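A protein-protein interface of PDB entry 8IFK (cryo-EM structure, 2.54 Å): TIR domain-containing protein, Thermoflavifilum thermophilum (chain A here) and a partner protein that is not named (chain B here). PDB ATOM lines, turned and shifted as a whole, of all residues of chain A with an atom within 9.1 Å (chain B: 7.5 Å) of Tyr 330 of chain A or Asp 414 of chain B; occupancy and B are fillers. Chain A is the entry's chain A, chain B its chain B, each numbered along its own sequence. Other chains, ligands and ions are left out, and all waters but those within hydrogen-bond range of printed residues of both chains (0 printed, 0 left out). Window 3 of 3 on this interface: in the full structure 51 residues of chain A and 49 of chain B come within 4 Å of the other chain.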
ATOM      1  N   TRP A 175      30.686  21.012 -22.628  1.00  0.00           N
ATOM      2  CA  TRP A 175      31.533  22.038 -22.034  1.00  0.00           C
ATOM      3  C   TRP A 175      32.845  21.413 -21.585  1.00  0.00           C
ATOM      4  O   TRP A 175      32.849  20.511 -20.741  1.00  0.00           O
ATOM      5  CB  TRP A 175      30.830  22.692 -20.845  1.00  0.00           C
ATOM      6  CG  TRP A 175      29.537  23.361 -21.187  1.00  0.00           C
ATOM      7  CD1 TRP A 175      28.973  23.477 -22.421  1.00  0.00           C
ATOM      8  CD2 TRP A 175      28.640  24.000 -20.274  1.00  0.00           C
ATOM      9  NE1 TRP A 175      27.783  24.155 -22.337  1.00  0.00           N
ATOM     10  CE2 TRP A 175      27.555  24.488 -21.028  1.00  0.00           C
ATOM     11  CE3 TRP A 175      28.649  24.210 -18.893  1.00  0.00           C
ATOM     12  CZ2 TRP A 175      26.490  25.170 -20.447  1.00  0.00           C
ATOM     13  CZ3 TRP A 175      27.593  24.889 -18.318  1.00  0.00           C
ATOM     14  CH2 TRP A 175      26.529  25.360 -19.094  1.00  0.00           C
ATOM     15  N   ILE A 178      38.108  25.220 -18.907  1.00  0.00           N
ATOM     16  CA  ILE A 178      39.375  25.910 -19.113  1.00  0.00           C
ATOM     17  C   ILE A 178      40.214  25.684 -17.861  1.00  0.00           C
ATOM     18  O   ILE A 178      39.910  26.225 -16.795  1.00  0.00           O
ATOM     19  CB  ILE A 178      39.173  27.403 -19.390  1.00  0.00           C
ATOM     20  CG1 ILE A 178      38.359  27.602 -20.668  1.00  0.00           C
ATOM     21  CG2 ILE A 178      40.517  28.093 -19.520  1.00  0.00           C
ATOM     22  CD1 ILE A 178      37.740  28.973 -20.795  1.00  0.00           C
ATOM     23  N   LEU A 247      37.692  37.082 -13.667  1.00  0.00           N
ATOM     24  CA  LEU A 247      36.732  35.983 -13.678  1.00  0.00           C
ATOM     25  C   LEU A 247      35.890  35.935 -12.411  1.00  0.00           C
ATOM     26  O   LEU A 247      34.729  35.514 -12.461  1.00  0.00           O
ATOM     27  CB  LEU A 247      37.456  34.651 -13.873  1.00  0.00           C
ATOM     28  CG  LEU A 247      38.405  34.578 -15.068  1.00  0.00           C
ATOM     29  CD1 LEU A 247      39.226  33.305 -15.012  1.00  0.00           C
ATOM     30  CD2 LEU A 247      37.635  34.671 -16.371  1.00  0.00           C
ATOM     31  N   SER A 248      36.446  36.354 -11.274  1.00  0.00           N
ATOM     32  CA  SER A 248      35.695  36.379 -10.028  1.00  0.00           C
ATOM     33  C   SER A 248      34.842  37.630  -9.877  1.00  0.00           C
ATOM     34  O   SER A 248      34.112  37.744  -8.887  1.00  0.00           O
ATOM     35  CB  SER A 248      36.648  36.272  -8.836  1.00  0.00           C
ATOM     36  OG  SER A 248      37.301  37.507  -8.602  1.00  0.00           O
ATOM     37  N   GLN A 262      35.460  40.490 -18.960  1.00  0.00           N
ATOM     38  CA  GLN A 262      35.163  39.085 -19.224  1.00  0.00           C
ATOM     39  C   GLN A 262      34.831  38.858 -20.693  1.00  0.00           C
ATOM     40  O   GLN A 262      35.199  37.827 -21.267  1.00  0.00           O
ATOM     41  CB  GLN A 262      34.018  38.615 -18.329  1.00  0.00           C
ATOM     42  CG  GLN A 262      34.339  38.658 -16.845  1.00  0.00           C
ATOM     43  CD  GLN A 262      33.410  37.791 -16.022  1.00  0.00           C
ATOM     44  OE1 GLN A 262      32.431  37.250 -16.532  1.00  0.00           O
ATOM     45  NE2 GLN A 262      33.716  37.650 -14.738  1.00  0.00           N
ATOM     46  N   VAL A 266      36.804  36.388 -23.211  1.00  0.00           N
ATOM     47  CA  VAL A 266      36.165  35.381 -24.055  1.00  0.00           C
ATOM     48  C   VAL A 266      36.537  35.587 -25.519  1.00  0.00           C
ATOM     49  O   VAL A 266      36.741  34.620 -26.263  1.00  0.00           O
ATOM     50  CB  VAL A 266      34.641  35.398 -23.845  1.00  0.00           C
ATOM     51  CG1 VAL A 266      33.938  34.776 -25.033  1.00  0.00           C
ATOM     52  CG2 VAL A 266      34.291  34.639 -22.587  1.00  0.00           C
ATOM     53  N   GLY A 327      34.172  30.145 -26.255  1.00  0.00           N
ATOM     54  CA  GLY A 327      34.526  30.263 -24.853  1.00  0.00           C
ATOM     55  C   GLY A 327      33.430  30.954 -24.060  1.00  0.00           C
ATOM     56  O   GLY A 327      32.781  31.887 -24.537  1.00  0.00           O
ATOM     57  N   LYS A 328      33.216  30.481 -22.833  1.00  0.00           N
ATOM     58  CA  LYS A 328      32.244  31.075 -21.926  1.00  0.00           C
ATOM     59  C   LYS A 328      32.810  31.038 -20.514  1.00  0.00           C
ATOM     60  O   LYS A 328      33.723  30.265 -20.221  1.00  0.00           O
ATOM     61  CB  LYS A 328      30.897  30.347 -21.976  1.00  0.00           C
ATOM     62  CG  LYS A 328      30.218  30.386 -23.335  1.00  0.00           C
ATOM     63  CD  LYS A 328      29.552  31.716 -23.619  1.00  0.00           C
ATOM     64  CE  LYS A 328      29.359  31.911 -25.115  1.00  0.00           C
ATOM     65  NZ  LYS A 328      28.406  30.927 -25.697  1.00  0.00           N
ATOM     66  N   LEU A 329      32.268  31.888 -19.641  1.00  0.00           N
ATOM     67  CA  LEU A 329      32.796  32.036 -18.291  1.00  0.00           C
ATOM     68  C   LEU A 329      31.722  32.080 -17.209  1.00  0.00           C
ATOM     69  O   LEU A 329      32.065  32.220 -16.031  1.00  0.00           O
ATOM     70  CB  LEU A 329      33.659  33.298 -18.193  1.00  0.00           C
ATOM     71  CG  LEU A 329      34.778  33.524 -19.208  1.00  0.00           C
ATOM     72  CD1 LEU A 329      35.274  34.958 -19.125  1.00  0.00           C
ATOM     73  CD2 LEU A 329      35.920  32.548 -18.986  1.00  0.00           C
ATOM     74  N   TYR A 330      30.438  31.975 -17.564  1.00  0.00           N
ATOM     75  CA  TYR A 330      29.422  32.229 -16.546  1.00  0.00           C
ATOM     76  C   TYR A 330      29.426  31.157 -15.455  1.00  0.00           C
ATOM     77  O   TYR A 330      29.723  31.484 -14.298  1.00  0.00           O
ATOM     78  CB  TYR A 330      28.023  32.368 -17.162  1.00  0.00           C
ATOM     79  CG  TYR A 330      26.921  32.093 -16.160  1.00  0.00           C
ATOM     80  CD1 TYR A 330      26.831  32.819 -14.978  1.00  0.00           C
ATOM     81  CD2 TYR A 330      25.993  31.084 -16.380  1.00  0.00           C
ATOM     82  CE1 TYR A 330      25.845  32.557 -14.054  1.00  0.00           C
ATOM     83  CE2 TYR A 330      25.001  30.819 -15.463  1.00  0.00           C
ATOM     84  CZ  TYR A 330      24.932  31.557 -14.301  1.00  0.00           C
ATOM     85  OH  TYR A 330      23.947  31.294 -13.380  1.00  0.00           O
ATOM     86  N   PRO A 331      29.103  29.873 -15.743  1.00  0.00           N
ATOM     87  CA  PRO A 331      29.070  28.893 -14.648  1.00  0.00           C
ATOM     88  C   PRO A 331      30.475  28.614 -14.150  1.00  0.00           C
ATOM     89  O   PRO A 331      30.758  28.638 -12.948  1.00  0.00           O
ATOM     90  CB  PRO A 331      28.443  27.649 -15.297  1.00  0.00           C
ATOM     91  CG  PRO A 331      27.935  28.108 -16.643  1.00  0.00           C
ATOM     92  CD  PRO A 331      28.866  29.204 -17.033  1.00  0.00           C
ATOM     93  N   SER A 332      31.359  28.352 -15.103  1.00  0.00           N
ATOM     94  CA  SER A 332      32.790  28.225 -14.888  1.00  0.00           C
ATOM     95  C   SER A 332      33.465  28.453 -16.228  1.00  0.00           C
ATOM     96  O   SER A 332      32.836  28.272 -17.277  1.00  0.00           O
ATOM     97  CB  SER A 332      33.156  26.846 -14.321  1.00  0.00           C
ATOM     98  OG  SER A 332      32.454  25.816 -14.993  1.00  0.00           O
ATOM     99  N   PRO A 333      34.727  28.875 -16.234  1.00  0.00           N
ATOM    100  CA  PRO A 333      35.424  29.051 -17.514  1.00  0.00           C
ATOM    101  C   PRO A 333      35.474  27.740 -18.282  1.00  0.00           C
ATOM    102  O   PRO A 333      36.155  26.792 -17.884  1.00  0.00           O
ATOM    103  CB  PRO A 333      36.819  29.521 -17.095  1.00  0.00           C
ATOM    104  CG  PRO A 333      36.620  30.137 -15.755  1.00  0.00           C
ATOM    105  CD  PRO A 333      35.541  29.331 -15.095  1.00  0.00           C
ATOM    106  N   VAL A 334      34.737  27.690 -19.389  1.00  0.00           N
ATOM    107  CA  VAL A 334      34.595  26.480 -20.190  1.00  0.00           C
ATOM    108  C   VAL A 334      34.631  26.856 -21.666  1.00  0.00           C
ATOM    109  O   VAL A 334      34.571  28.029 -22.042  1.00  0.00           O
ATOM    110  CB  VAL A 334      33.292  25.708 -19.876  1.00  0.00           C
ATOM    111  CG1 VAL A 334      33.331  25.130 -18.471  1.00  0.00           C
ATOM    112  CG2 VAL A 334      32.080  26.606 -20.066  1.00  0.00           C
ATOM    113  N   LEU A 335      34.728  25.833 -22.505  1.00  0.00           N
ATOM    114  CA  LEU A 335      34.660  25.957 -23.951  1.00  0.00           C
ATOM    115  C   LEU A 335      33.516  25.075 -24.429  1.00  0.00           C
ATOM    116  O   LEU A 335      33.563  23.852 -24.260  1.00  0.00           O
ATOM    117  CB  LEU A 335      35.989  25.537 -24.581  1.00  0.00           C
ATOM    118  CG  LEU A 335      36.301  25.890 -26.031  1.00  0.00           C
ATOM    119  CD1 LEU A 335      36.771  27.328 -26.146  1.00  0.00           C
ATOM    120  CD2 LEU A 335      37.361  24.940 -26.560  1.00  0.00           C
ATOM    121  N   MET A 336      32.471  25.696 -24.973  1.00  0.00           N
ATOM    122  CA  MET A 336      31.334  24.954 -25.498  1.00  0.00           C
ATOM    123  C   MET A 336      31.644  24.530 -26.925  1.00  0.00           C
ATOM    124  O   MET A 336      31.924  25.376 -27.783  1.00  0.00           O
ATOM    125  CB  MET A 336      30.065  25.800 -25.447  1.00  0.00           C
ATOM    126  CG  MET A 336      29.671  26.230 -24.047  1.00  0.00           C
ATOM    127  SD  MET A 336      28.464  27.560 -24.017  1.00  0.00           S
ATOM    128  CE  MET A 336      28.155  27.697 -22.259  1.00  0.00           C
ATOM    129  N   LEU A 408      32.986  18.662 -18.932  1.00  0.00           N
ATOM    130  CA  LEU A 408      32.353  18.705 -17.622  1.00  0.00           C
ATOM    131  C   LEU A 408      31.481  17.473 -17.422  1.00  0.00           C
ATOM    132  O   LEU A 408      30.713  17.083 -18.305  1.00  0.00           O
ATOM    133  CB  LEU A 408      31.514  19.973 -17.472  1.00  0.00           C
ATOM    134  CG  LEU A 408      32.248  21.259 -17.096  1.00  0.00           C
ATOM    135  CD1 LEU A 408      31.287  22.430 -17.120  1.00  0.00           C
ATOM    136  CD2 LEU A 408      32.879  21.117 -15.724  1.00  0.00           C
ATOM    137  N   LYS B 392      20.907  26.797 -26.556  1.00  0.00           N
ATOM    138  CA  LYS B 392      22.101  27.226 -25.844  1.00  0.00           C
ATOM    139  C   LYS B 392      23.090  26.067 -25.831  1.00  0.00           C
ATOM    140  O   LYS B 392      22.734  24.962 -25.405  1.00  0.00           O
ATOM    141  CB  LYS B 392      21.770  27.673 -24.422  1.00  0.00           C
ATOM    142  CG  LYS B 392      22.573  28.882 -23.964  1.00  0.00           C
ATOM    143  CD  LYS B 392      21.803  29.729 -22.966  1.00  0.00           C
ATOM    144  CE  LYS B 392      22.741  30.523 -22.069  1.00  0.00           C
ATOM    145  NZ  LYS B 392      23.351  29.681 -21.003  1.00  0.00           N
ATOM    146  N   TYR B 411      19.761  20.526 -14.969  1.00  0.00           N
ATOM    147  CA  TYR B 411      21.001  21.029 -14.395  1.00  0.00           C
ATOM    148  C   TYR B 411      20.724  22.391 -13.774  1.00  0.00           C
ATOM    149  O   TYR B 411      20.430  23.354 -14.490  1.00  0.00           O
ATOM    150  CB  TYR B 411      22.093  21.126 -15.462  1.00  0.00           C
ATOM    151  CG  TYR B 411      23.368  21.794 -14.995  1.00  0.00           C
ATOM    152  CD1 TYR B 411      23.845  21.606 -13.703  1.00  0.00           C
ATOM    153  CD2 TYR B 411      24.096  22.610 -15.848  1.00  0.00           C
ATOM    154  CE1 TYR B 411      25.006  22.216 -13.277  1.00  0.00           C
ATOM    155  CE2 TYR B 411      25.261  23.222 -15.430  1.00  0.00           C
ATOM    156  CZ  TYR B 411      25.711  23.023 -14.144  1.00  0.00           C
ATOM    157  OH  TYR B 411      26.869  23.633 -13.724  1.00  0.00           O
ATOM    158  N   ILE B 412      20.826  22.471 -12.453  1.00  0.00           N
ATOM    159  CA  ILE B 412      20.539  23.691 -11.706  1.00  0.00           C
ATOM    160  C   ILE B 412      21.839  24.483 -11.634  1.00  0.00           C
ATOM    161  O   ILE B 412      22.670  24.262 -10.748  1.00  0.00           O
ATOM    162  CB  ILE B 412      19.981  23.386 -10.314  1.00  0.00           C
ATOM    163  CG1 ILE B 412      18.664  22.619 -10.426  1.00  0.00           C
ATOM    164  CG2 ILE B 412      19.766  24.671  -9.531  1.00  0.00           C
ATOM    165  CD1 ILE B 412      17.511  23.461 -10.899  1.00  0.00           C
ATOM    166  N   VAL B 413      22.026  25.402 -12.582  1.00  0.00           N
ATOM    167  CA  VAL B 413      23.242  26.211 -12.602  1.00  0.00           C
ATOM    168  C   VAL B 413      23.256  27.177 -11.424  1.00  0.00           C
ATOM    169  O   VAL B 413      24.257  27.304 -10.710  1.00  0.00           O
ATOM    170  CB  VAL B 413      23.367  26.959 -13.940  1.00  0.00           C
ATOM    171  CG1 VAL B 413      24.701  27.676 -14.019  1.00  0.00           C
ATOM    172  CG2 VAL B 413      23.189  26.002 -15.105  1.00  0.00           C
ATOM    173  N   ASP B 414      22.140  27.869 -11.202  1.00  0.00           N
ATOM    174  CA  ASP B 414      22.030  28.874 -10.157  1.00  0.00           C
ATOM    175  C   ASP B 414      20.672  28.736  -9.485  1.00  0.00           C
ATOM    176  O   ASP B 414      19.848  27.898  -9.863  1.00  0.00           O
ATOM    177  CB  ASP B 414      22.215  30.285 -10.726  1.00  0.00           C
ATOM    178  CG  ASP B 414      23.556  30.889 -10.369  1.00  0.00           C
ATOM    179  OD1 ASP B 414      24.382  30.185  -9.751  1.00  0.00           O
ATOM    180  OD2 ASP B 414      23.784  32.069 -10.706  1.00  0.00           O
ATOM    181  N   GLU B 415      20.437  29.575  -8.474  1.00  0.00           N
ATOM    182  CA  GLU B 415      19.109  29.647  -7.876  1.00  0.00           C
ATOM    183  C   GLU B 415      18.098  30.248  -8.843  1.00  0.00           C
ATOM    184  O   GLU B 415      16.888  30.080  -8.657  1.00  0.00           O
ATOM    185  CB  GLU B 415      19.155  30.460  -6.581  1.00  0.00           C
ATOM    186  CG  GLU B 415      19.793  29.747  -5.392  1.00  0.00           C
ATOM    187  CD  GLU B 415      18.908  28.666  -4.792  1.00  0.00           C
ATOM    188  OE1 GLU B 415      18.529  27.719  -5.513  1.00  0.00           O
ATOM    189  OE2 GLU B 415      18.588  28.767  -3.589  1.00  0.00           O
ATOM    190  N   LYS B 416      18.574  30.949  -9.873  1.00  0.00           N
ATOM    191  CA  LYS B 416      17.712  31.562 -10.871  1.00  0.00           C
ATOM    192  C   LYS B 416      17.904  31.003 -12.272  1.00  0.00           C
ATOM    193  O   LYS B 416      17.006  31.156 -13.105  1.00  0.00           O
ATOM    194  CB  LYS B 416      17.942  33.081 -10.911  1.00  0.00           C
ATOM    195  CG  LYS B 416      17.169  33.857  -9.859  1.00  0.00           C
ATOM    196  CD  LYS B 416      17.822  35.200  -9.576  1.00  0.00           C
ATOM    197  CE  LYS B 416      17.228  35.858  -8.342  1.00  0.00           C
ATOM    198  NZ  LYS B 416      15.974  35.189  -7.897  1.00  0.00           N
ATOM    199  N   LYS B 417      19.036  30.362 -12.550  1.00  0.00           N
ATOM    200  CA  LYS B 417      19.347  29.831 -13.869  1.00  0.00           C
ATOM    201  C   LYS B 417      19.486  28.318 -13.804  1.00  0.00           C
ATOM    202  O   LYS B 417      20.029  27.774 -12.837  1.00  0.00           O
ATOM    203  CB  LYS B 417      20.634  30.449 -14.421  1.00  0.00           C
ATOM    204  CG  LYS B 417      20.449  31.849 -14.965  1.00  0.00           C
ATOM    205  CD  LYS B 417      21.609  32.761 -14.623  1.00  0.00           C
ATOM    206  CE  LYS B 417      21.935  33.699 -15.771  1.00  0.00           C
ATOM    207  NZ  LYS B 417      22.886  33.079 -16.735  1.00  0.00           N
ATOM    208  N   ALA B 418      18.993  27.640 -14.839  1.00  0.00           N
ATOM    209  CA  ALA B 418      19.077  26.189 -14.899  1.00  0.00           C
ATOM    210  C   ALA B 418      18.913  25.734 -16.341  1.00  0.00           C
ATOM    211  O   ALA B 418      18.487  26.498 -17.210  1.00  0.00           O
ATOM    212  CB  ALA B 418      18.023  25.527 -14.008  1.00  0.00           C
ATOM    213  N   PHE B 419      19.280  24.482 -16.583  1.00  0.00           N
ATOM    214  CA  PHE B 419      18.999  23.798 -17.837  1.00  0.00           C
ATOM    215  C   PHE B 419      17.935  22.740 -17.587  1.00  0.00           C
ATOM    216  O   PHE B 419      17.997  22.015 -16.591  1.00  0.00           O
ATOM    217  CB  PHE B 419      20.257  23.139 -18.404  1.00  0.00           C
ATOM    218  CG  PHE B 419      21.216  24.099 -19.039  1.00  0.00           C
ATOM    219  CD1 PHE B 419      21.082  24.454 -20.370  1.00  0.00           C
ATOM    220  CD2 PHE B 419      22.255  24.647 -18.306  1.00  0.00           C
ATOM    221  CE1 PHE B 419      21.965  25.335 -20.958  1.00  0.00           C
ATOM    222  CE2 PHE B 419      23.139  25.529 -18.889  1.00  0.00           C
ATOM    223  CZ  PHE B 419      22.995  25.873 -20.217  1.00  0.00           C
ATOM    224  N   PHE B 442      17.404  26.528 -21.728  1.00  0.00           N
ATOM    225  CA  PHE B 442      17.963  27.278 -20.614  1.00  0.00           C
ATOM    226  C   PHE B 442      16.882  28.173 -20.027  1.00  0.00           C
ATOM    227  O   PHE B 442      16.366  29.062 -20.711  1.00  0.00           O
ATOM    228  CB  PHE B 442      19.163  28.104 -21.067  1.00  0.00           C
ATOM    229  CG  PHE B 442      19.897  28.767 -19.942  1.00  0.00           C
ATOM    230  CD1 PHE B 442      20.582  28.011 -19.007  1.00  0.00           C
ATOM    231  CD2 PHE B 442      19.902  30.145 -19.816  1.00  0.00           C
ATOM    232  CE1 PHE B 442      21.257  28.616 -17.970  1.00  0.00           C
ATOM    233  CE2 PHE B 442      20.577  30.754 -18.780  1.00  0.00           C
ATOM    234  CZ  PHE B 442      21.256  29.988 -17.857  1.00  0.00           C
ATOM    235  N   ILE B 443      16.537  27.936 -18.767  1.00  0.00           N
ATOM    236  CA  ILE B 443      15.488  28.673 -18.080  1.00  0.00           C
ATOM    237  C   ILE B 443      16.142  29.549 -17.024  1.00  0.00           C
ATOM    238  O   ILE B 443      16.792  29.044 -16.099  1.00  0.00           O
ATOM    239  CB  ILE B 443      14.450  27.727 -17.461  1.00  0.00           C
ATOM    240  CG1 ILE B 443      13.556  27.155 -18.560  1.00  0.00           C
ATOM    241  CG2 ILE B 443      13.630  28.447 -16.405  1.00  0.00           C
ATOM    242  CD1 ILE B 443      13.412  25.663 -18.511  1.00  0.00           C
ATOM    243  N   GLU B 444      15.971  30.857 -17.164  1.00  0.00           N
ATOM    244  CA  GLU B 444      16.489  31.836 -16.225  1.00  0.00           C
ATOM    245  C   GLU B 444      15.335  32.528 -15.518  1.00  0.00           C
ATOM    246  O   GLU B 444      14.363  32.940 -16.157  1.00  0.00           O
ATOM    247  CB  GLU B 444      17.353  32.877 -16.942  1.00  0.00           C
ATOM    248  CG  GLU B 444      17.961  33.917 -16.020  1.00  0.00           C
ATOM    249  CD  GLU B 444      18.444  35.143 -16.762  1.00  0.00           C
ATOM    250  OE1 GLU B 444      18.779  35.022 -17.959  1.00  0.00           O
ATOM    251  OE2 GLU B 444      18.496  36.229 -16.147  1.00  0.00           O
ATOM    252  N   ILE B 445      15.443  32.660 -14.200  1.00  0.00           N
ATOM    253  CA  ILE B 445      14.512  33.515 -13.479  1.00  0.00           C
ATOM    254  C   ILE B 445      15.100  34.916 -13.548  1.00  0.00           C
ATOM    255  O   ILE B 445      15.786  35.367 -12.625  1.00  0.00           O
ATOM    256  CB  ILE B 445      14.292  33.045 -12.030  1.00  0.00           C
ATOM    257  CG1 ILE B 445      13.723  31.626 -12.018  1.00  0.00           C
ATOM    258  CG2 ILE B 445      13.333  33.974 -11.304  1.00  0.00           C
ATOM    259  CD1 ILE B 445      13.846  30.936 -10.681  1.00  0.00           C
ATOM    260  N   ILE B 452      13.686  27.630  -8.413  1.00  0.00           N
ATOM    261  CA  ILE B 452      14.022  27.218  -9.772  1.00  0.00           C
ATOM    262  C   ILE B 452      13.484  25.822 -10.063  1.00  0.00           C
ATOM    263  O   ILE B 452      13.038  25.537 -11.181  1.00  0.00           O
ATOM    264  CB  ILE B 452      15.544  27.314  -9.998  1.00  0.00           C
ATOM    265  CG1 ILE B 452      15.891  26.999 -11.454  1.00  0.00           C
ATOM    266  CG2 ILE B 452      16.304  26.413  -9.034  1.00  0.00           C
ATOM    267  CD1 ILE B 452      15.273  27.952 -12.453  1.00  0.00           C
ATOM    268  N   GLN B 453      13.502  24.934  -9.065  1.00  0.00           N
ATOM    269  CA  GLN B 453      12.964  23.592  -9.264  1.00  0.00           C
ATOM    270  C   GLN B 453      11.475  23.638  -9.575  1.00  0.00           C
ATOM    271  O   GLN B 453      10.993  22.918 -10.458  1.00  0.00           O
ATOM    272  CB  GLN B 453      13.231  22.733  -8.029  1.00  0.00           C
ATOM    273  CG  GLN B 453      14.577  22.995  -7.374  1.00  0.00           C
ATOM    274  CD  GLN B 453      15.399  21.732  -7.207  1.00  0.00           C
ATOM    275  OE1 GLN B 453      14.863  20.624  -7.207  1.00  0.00           O
ATOM    276  NE2 GLN B 453      16.709  21.895  -7.063  1.00  0.00           N
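The side-chain carboxylate (OD2) of Asp 414 of chain B is in hydrogen-bond range of the side-chain hydroxyl (OH) of Tyr 330 of chain A (2.8 Å).
The backbone carbonyl oxygen (O) of Trp 175 of chain A is in hydrogen-bond range of the backbone NH (N) of Leu 408 of chain A (2.6 Å).
The backbone carbonyl oxygen (O) of Tyr 411 of chain B sits at hydrogen-bond distance from the backbone NH (N) of Phe 419 of chain B.
Among the printed residues, pairs that only touch across the chains: Trp 175 of chain A with Phe 419 of chain B (3.4 Å), Tyr 330 of chain A with Val 413 of chain B (3.5 Å), Tyr 330 of chain A with Lys 417 of chain B (3.0 Å) and Pro 331 of chain A with Val 413 of chain B (3.95 Å).
Of chain A, only Tyr 330 comes within 4 Å of Asp 414 of chain B.
Printed residues of chain A within 4 Å of Lys 417 of chain B: Tyr 330.
Of the printed residues of chain B, Trp 175 of chain A touches Phe 419 (3.4 Å).
Printed residues of chain A within 4 Å of Phe 419 of chain B: Trp 175 (3.4 Å).
Lys 392 of chain B touches none of the printed residues of chain A.
The nearest printed residue of chain B that does not touch Trp 175 of chain A is Tyr 411 of chain B (4.1 Å).
Hydrophobic or aromatic side chains of chain A that line the printed part of chain B: Trp 175, Tyr 330 and Pro 331.
Along chain A the printed residues that touch a printed residue of chain B span positions 175 to 331.
Of the 16 printed residues of chain B, 4 touch a printed residue of chain A.
Hydrophobic or aromatic side chains of chain B within 4 Å of the printed part of chain A: Val 413 and Phe 419.
Along chain B the printed residues that touch a printed residue of chain A span positions 413 to 419.
Among the printed residues, no Asp or Glu carboxylate lies within 4 Å of a Lys or Arg side-chain nitrogen of the other chain.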
